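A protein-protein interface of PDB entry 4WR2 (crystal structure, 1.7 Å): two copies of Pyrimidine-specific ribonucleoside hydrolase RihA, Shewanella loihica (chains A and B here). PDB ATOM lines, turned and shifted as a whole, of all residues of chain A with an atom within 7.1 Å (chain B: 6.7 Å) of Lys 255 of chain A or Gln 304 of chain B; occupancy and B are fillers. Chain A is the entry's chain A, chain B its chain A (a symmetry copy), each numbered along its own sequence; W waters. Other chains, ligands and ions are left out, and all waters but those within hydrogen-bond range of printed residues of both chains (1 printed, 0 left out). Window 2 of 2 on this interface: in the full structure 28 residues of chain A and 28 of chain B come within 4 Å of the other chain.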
ATOM      1  N   ASN A 182     -17.444  23.385   1.055  1.00  0.00           N
ATOM      2  CA  ASN A 182     -18.653  24.114   1.433  1.00  0.00           C
ATOM      3  C   ASN A 182     -18.375  25.378   2.251  1.00  0.00           C
ATOM      4  O   ASN A 182     -19.328  26.084   2.634  1.00  0.00           O
ATOM      5  CB  ASN A 182     -19.583  23.194   2.232  1.00  0.00           C
ATOM      6  CG  ASN A 182     -19.034  22.834   3.605  1.00  0.00           C
ATOM      7  OD1 ASN A 182     -17.858  23.002   3.885  1.00  0.00           O
ATOM      8  ND2 ASN A 182     -19.906  22.334   4.467  1.00  0.00           N
ATOM      9  N   PRO A 185     -14.059  27.426  -1.703  1.00  0.00           N
ATOM     10  CA  PRO A 185     -14.317  26.547  -2.844  1.00  0.00           C
ATOM     11  C   PRO A 185     -13.578  25.224  -2.734  1.00  0.00           C
ATOM     12  O   PRO A 185     -14.040  24.230  -3.270  1.00  0.00           O
ATOM     13  CB  PRO A 185     -13.810  27.366  -4.026  1.00  0.00           C
ATOM     14  CG  PRO A 185     -14.087  28.789  -3.604  1.00  0.00           C
ATOM     15  CD  PRO A 185     -13.710  28.788  -2.137  1.00  0.00           C
ATOM     16  N   ARG A 252     -31.060  24.150   3.268  1.00  0.00           N
ATOM     17  CA  ARG A 252     -31.344  23.834   1.868  1.00  0.00           C
ATOM     18  C   ARG A 252     -31.227  25.062   0.966  1.00  0.00           C
ATOM     19  O   ARG A 252     -32.116  25.337   0.148  1.00  0.00           O
ATOM     20  CB  ARG A 252     -32.731  23.203   1.724  1.00  0.00           C
ATOM     21  CG  ARG A 252     -32.806  21.780   2.245  1.00  0.00           C
ATOM     22  CD  ARG A 252     -34.014  21.062   1.684  1.00  0.00           C
ATOM     23  NE  ARG A 252     -35.258  21.735   2.047  1.00  0.00           N
ATOM     24  CZ  ARG A 252     -36.455  21.405   1.585  1.00  0.00           C
ATOM     25  NH1 ARG A 252     -36.587  20.401   0.723  1.00  0.00           N
ATOM     26  NH2 ARG A 252     -37.533  22.071   1.987  1.00  0.00           N
ATOM     27  N   ASP A 253     -30.128  25.801   1.124  1.00  0.00           N
ATOM     28  CA  ASP A 253     -29.838  26.917   0.217  1.00  0.00           C
ATOM     29  C   ASP A 253     -29.923  26.339  -1.197  1.00  0.00           C
ATOM     30  O   ASP A 253     -29.222  25.371  -1.495  1.00  0.00           O
ATOM     31  CB  ASP A 253     -28.455  27.508   0.505  1.00  0.00           C
ATOM     32  CG  ASP A 253     -28.145  28.745  -0.347  1.00  0.00           C
ATOM     33  OD1 ASP A 253     -28.598  28.837  -1.513  1.00  0.00           O
ATOM     34  OD2 ASP A 253     -27.421  29.632   0.159  1.00  0.00           O
ATOM     35  N   PRO A 254     -30.798  26.890  -2.043  1.00  0.00           N
ATOM     36  CA  PRO A 254     -31.023  26.279  -3.363  1.00  0.00           C
ATOM     37  C   PRO A 254     -29.764  26.124  -4.233  1.00  0.00           C
ATOM     38  O   PRO A 254     -29.775  25.319  -5.167  1.00  0.00           O
ATOM     39  CB  PRO A 254     -31.986  27.253  -4.038  1.00  0.00           C
ATOM     40  CG  PRO A 254     -32.677  27.927  -2.886  1.00  0.00           C
ATOM     41  CD  PRO A 254     -31.582  28.133  -1.894  1.00  0.00           C
ATOM     42  N   LYS A 255     -28.708  26.880  -3.941  1.00  0.00           N
ATOM     43  CA  LYS A 255     -27.502  26.823  -4.776  1.00  0.00           C
ATOM     44  C   LYS A 255     -26.859  25.443  -4.723  1.00  0.00           C
ATOM     45  O   LYS A 255     -26.198  25.029  -5.674  1.00  0.00           O
ATOM     46  CB  LYS A 255     -26.497  27.896  -4.364  1.00  0.00           C
ATOM     47  CG  LYS A 255     -25.877  27.711  -2.998  1.00  0.00           C
ATOM     48  CD  LYS A 255     -25.043  28.934  -2.645  1.00  0.00           C
ATOM     49  CE  LYS A 255     -24.208  28.733  -1.389  1.00  0.00           C
ATOM     50  NZ  LYS A 255     -23.463  29.983  -1.066  1.00  0.00           N
ATOM     51  N   TRP A 256     -27.083  24.728  -3.623  1.00  0.00           N
ATOM     52  CA  TRP A 256     -26.508  23.397  -3.448  1.00  0.00           C
ATOM     53  C   TRP A 256     -27.274  22.347  -4.240  1.00  0.00           C
ATOM     54  O   TRP A 256     -26.738  21.279  -4.544  1.00  0.00           O
ATOM     55  CB  TRP A 256     -26.481  23.000  -1.969  1.00  0.00           C
ATOM     56  CG  TRP A 256     -25.661  23.902  -1.120  1.00  0.00           C
ATOM     57  CD1 TRP A 256     -26.107  24.714  -0.118  1.00  0.00           C
ATOM     58  CD2 TRP A 256     -24.238  24.103  -1.202  1.00  0.00           C
ATOM     59  NE1 TRP A 256     -25.050  25.399   0.441  1.00  0.00           N
ATOM     60  CE2 TRP A 256     -23.896  25.047  -0.212  1.00  0.00           C
ATOM     61  CE3 TRP A 256     -23.232  23.569  -2.007  1.00  0.00           C
ATOM     62  CZ2 TRP A 256     -22.582  25.473  -0.007  1.00  0.00           C
ATOM     63  CZ3 TRP A 256     -21.917  23.983  -1.792  1.00  0.00           C
ATOM     64  CH2 TRP A 256     -21.611  24.930  -0.806  1.00  0.00           C
ATOM     65  N   GLY A 257     -28.535  22.646  -4.546  1.00  0.00           N
ATOM     66  CA  GLY A 257     -29.397  21.727  -5.282  1.00  0.00           C
ATOM     67  C   GLY A 257     -29.824  20.492  -4.496  1.00  0.00           C
ATOM     68  O   GLY A 257     -30.008  19.425  -5.073  1.00  0.00           O
ATOM     69  N   PHE A 258     -29.964  20.628  -3.182  1.00  0.00           N
ATOM     70  CA  PHE A 258     -30.464  19.535  -2.336  1.00  0.00           C
ATOM     71  C   PHE A 258     -31.975  19.346  -2.531  1.00  0.00           C
ATOM     72  O   PHE A 258     -32.713  20.322  -2.651  1.00  0.00           O
ATOM     73  CB  PHE A 258     -30.246  19.846  -0.867  1.00  0.00           C
ATOM     74  CG  PHE A 258     -28.802  19.891  -0.444  1.00  0.00           C
ATOM     75  CD1 PHE A 258     -27.949  18.845  -0.723  1.00  0.00           C
ATOM     76  CD2 PHE A 258     -28.308  20.997   0.236  1.00  0.00           C
ATOM     77  CE1 PHE A 258     -26.620  18.896  -0.324  1.00  0.00           C
ATOM     78  CE2 PHE A 258     -26.985  21.058   0.632  1.00  0.00           C
ATOM     79  CZ  PHE A 258     -26.141  20.008   0.351  1.00  0.00           C
ATOM     80  N   GLN B 281     -21.534  29.192 -16.261  1.00  0.00           N
ATOM     81  CA  GLN B 281     -21.773  30.080 -15.131  1.00  0.00           C
ATOM     82  C   GLN B 281     -20.599  31.033 -14.966  1.00  0.00           C
ATOM     83  O   GLN B 281     -19.457  30.630 -15.093  1.00  0.00           O
ATOM     84  CB  GLN B 281     -21.983  29.259 -13.860  1.00  0.00           C
ATOM     85  CG  GLN B 281     -22.305  30.076 -12.627  1.00  0.00           C
ATOM     86  CD  GLN B 281     -22.425  29.188 -11.401  1.00  0.00           C
ATOM     87  OE1 GLN B 281     -23.040  28.112 -11.466  1.00  0.00           O
ATOM     88  NE2 GLN B 281     -21.843  29.619 -10.300  1.00  0.00           N
ATOM     89  N   GLU B 282     -20.899  32.297 -14.687  1.00  0.00           N
ATOM     90  CA  GLU B 282     -19.881  33.273 -14.375  1.00  0.00           C
ATOM     91  C   GLU B 282     -19.368  33.001 -12.950  1.00  0.00           C
ATOM     92  O   GLU B 282     -20.156  32.997 -11.995  1.00  0.00           O
ATOM     93  CB  GLU B 282     -20.462  34.693 -14.432  1.00  0.00           C
ATOM     94  CG  GLU B 282     -21.047  35.085 -15.780  1.00  0.00           C
ATOM     95  CD  GLU B 282     -20.027  34.961 -16.879  1.00  0.00           C
ATOM     96  OE1 GLU B 282     -19.064  35.759 -16.876  1.00  0.00           O
ATOM     97  OE2 GLU B 282     -20.184  34.058 -17.722  1.00  0.00           O
ATOM     98  N   ASP B 301     -15.134  29.173  -7.750  1.00  0.00           N
ATOM     99  CA  ASP B 301     -16.131  29.508  -6.750  1.00  0.00           C
ATOM    100  C   ASP B 301     -17.538  29.387  -7.291  1.00  0.00           C
ATOM    101  O   ASP B 301     -18.311  30.353  -7.293  1.00  0.00           O
ATOM    102  CB  ASP B 301     -15.873  30.914  -6.209  1.00  0.00           C
ATOM    103  CG  ASP B 301     -16.704  31.237  -4.991  1.00  0.00           C
ATOM    104  OD1 ASP B 301     -17.217  30.296  -4.304  1.00  0.00           O
ATOM    105  OD2 ASP B 301     -16.846  32.446  -4.710  1.00  0.00           O
ATOM    106  N   ARG B 302     -17.896  28.166  -7.672  1.00  0.00           N
ATOM    107  CA  ARG B 302     -19.197  27.869  -8.252  1.00  0.00           C
ATOM    108  C   ARG B 302     -20.357  28.182  -7.310  1.00  0.00           C
ATOM    109  O   ARG B 302     -21.460  28.479  -7.775  1.00  0.00           O
ATOM    110  CB  ARG B 302     -19.248  26.397  -8.682  1.00  0.00           C
ATOM    111  CG  ARG B 302     -20.550  25.972  -9.331  1.00  0.00           C
ATOM    112  CD  ARG B 302     -20.573  24.480  -9.638  1.00  0.00           C
ATOM    113  NE  ARG B 302     -21.603  24.159 -10.633  1.00  0.00           N
ATOM    114  CZ  ARG B 302     -21.719  22.985 -11.249  1.00  0.00           C
ATOM    115  NH1 ARG B 302     -20.873  21.997 -10.976  1.00  0.00           N
ATOM    116  NH2 ARG B 302     -22.676  22.801 -12.150  1.00  0.00           N
ATOM    117  N   TYR B 303     -20.141  28.090  -5.995  1.00  0.00           N
ATOM    118  CA  TYR B 303     -21.211  28.240  -5.026  1.00  0.00           C
ATOM    119  C   TYR B 303     -21.172  29.579  -4.308  1.00  0.00           C
ATOM    120  O   TYR B 303     -21.876  29.773  -3.296  1.00  0.00           O
ATOM    121  CB  TYR B 303     -21.215  27.061  -4.040  1.00  0.00           C
ATOM    122  CG  TYR B 303     -21.490  25.773  -4.770  1.00  0.00           C
ATOM    123  CD1 TYR B 303     -22.773  25.457  -5.192  1.00  0.00           C
ATOM    124  CD2 TYR B 303     -20.460  24.907  -5.107  1.00  0.00           C
ATOM    125  CE1 TYR B 303     -23.029  24.308  -5.898  1.00  0.00           C
ATOM    126  CE2 TYR B 303     -20.709  23.756  -5.821  1.00  0.00           C
ATOM    127  CZ  TYR B 303     -21.994  23.460  -6.220  1.00  0.00           C
ATOM    128  OH  TYR B 303     -22.245  22.299  -6.919  1.00  0.00           O
ATOM    129  N   GLN B 304     -20.399  30.506  -4.872  1.00  0.00           N
ATOM    130  CA  GLN B 304     -20.369  31.900  -4.418  1.00  0.00           C
ATOM    131  C   GLN B 304     -20.114  31.993  -2.920  1.00  0.00           C
ATOM    132  O   GLN B 304     -20.904  32.560  -2.156  1.00  0.00           O
ATOM    133  CB  GLN B 304     -21.672  32.610  -4.779  1.00  0.00           C
ATOM    134  CG  GLN B 304     -21.901  32.682  -6.282  1.00  0.00           C
ATOM    135  CD  GLN B 304     -23.132  33.510  -6.631  1.00  0.00           C
ATOM    136  OE1 GLN B 304     -24.255  33.100  -6.397  1.00  0.00           O
ATOM    137  NE2 GLN B 304     -22.907  34.687  -7.190  1.00  0.00           N
ATOM    138  N   LEU B 305     -18.993  31.416  -2.518  1.00  0.00           N
ATOM    139  CA  LEU B 305     -18.587  31.393  -1.136  1.00  0.00           C
ATOM    140  C   LEU B 305     -17.617  32.512  -0.794  1.00  0.00           C
ATOM    141  O   LEU B 305     -17.464  32.825   0.382  1.00  0.00           O
ATOM    142  CB  LEU B 305     -17.932  30.038  -0.818  1.00  0.00           C
ATOM    143  CG  LEU B 305     -18.767  28.796  -1.129  1.00  0.00           C
ATOM    144  CD1 LEU B 305     -17.948  27.533  -0.914  1.00  0.00           C
ATOM    145  CD2 LEU B 305     -20.037  28.777  -0.287  1.00  0.00           C
ATOM    146  N   THR B 306     -16.932  33.080  -1.791  1.00  0.00           N
ATOM    147  CA  THR B 306     -15.812  34.002  -1.527  1.00  0.00           C
ATOM    148  C   THR B 306     -16.177  35.490  -1.571  1.00  0.00           C
ATOM    149  O   THR B 306     -15.428  36.321  -1.062  1.00  0.00           O
ATOM    150  CB  THR B 306     -14.667  33.825  -2.498  1.00  0.00           C
ATOM    151  OG1 THR B 306     -15.060  34.286  -3.804  1.00  0.00           O
ATOM    152  CG2 THR B 306     -14.209  32.344  -2.560  1.00  0.00           C
ATOM    153  N   GLY B 307     -17.289  35.814  -2.201  1.00  0.00           N
ATOM    154  CA  GLY B 307     -17.650  37.208  -2.425  1.00  0.00           C
ATOM    155  C   GLY B 307     -16.855  37.892  -3.529  1.00  0.00           C
ATOM    156  O   GLY B 307     -17.049  39.076  -3.779  1.00  0.00           O
HETATM  157  O   HOH W   1     -23.509  32.747  -1.680  1.00  0.00           O
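The side-chain amino group of Lys 255 of chain A sits at hydrogen-bond distance from the backbone carbonyl oxygen of Tyr 303 of chain B.
The side-chain carboxylate (OD1) of Asp 253 of chain A lies close to the backbone NH (N) of Lys 255 of chain A, 3.1 Å away.
The side-chain carboxylate (OD1) of Asp 301 of chain B lies within hydrogen-bond range of the backbone NH (N) of Gln 304 of chain B, 3.2 Å away.
OD1 of Asp 301 of chain B is in hydrogen-bond range of N of Leu 305 of chain B.
OD2 of Asp 301 of chain B is in hydrogen-bond range of OG1 of Thr 306 of chain B (2.7 Å).
Among the printed residues, merely in contact across the chains: Asn 182 of chain A with Leu 305 of chain B (3.9 Å), Pro 185 of chain A with Asp 301 of chain B (3.5 Å), Pro 185 of chain A with Leu 305 of chain B (3.97 Å), Pro 185 of chain A with Thr 306 of chain B (3.6 Å), Lys 255 of chain A with Gln 304 of chain B (3.8 Å), Lys 255 of chain A with Leu 305 of chain B (3.7 Å) and Trp 256 of chain A with Tyr 303 of chain B (3.5 Å).
Asp 253 of chain A touches none of the printed residues of chain B.
Of chain B, only Tyr 303, Gln 304 and Leu 305 come within 4 Å of Lys 255 of chain A.
Of the printed residues of chain B, Trp 256 of chain A touches Tyr 303 (3.5 Å).
Gln 281 of chain B touches none of the printed residues of chain A.
Of the printed residues of chain A, Asp 301 of chain B touches Pro 185.
Gln 304 of chain B touches just one residue of chain A: Lys 255 (3.8 Å).
The nearest residue of chain A that does not touch Gln 304 of chain B is Pro 185 of chain A (6.7 Å).
Of the 9 printed residues of chain B, 5 touch a printed residue of chain A.
Printed residues of chain A that touch a printed residue of chain B: Asn 182, Pro 185, Lys 255 and Trp 256.
Hydrophobic or aromatic side chains of chain A that line the printed part of chain B: Pro 185 and Trp 256.
Among the printed residues, no Asp or Glu carboxylate lies within 4 Å of a Lys or Arg side-chain nitrogen of the other chain.
No position is printed for both chains.
Water W1 bridges the backbone carbonyl oxygen of Gln 304 of chain B (2.7 Å) and the side-chain amino group of Lys 255 of chain A (2.8 Å).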
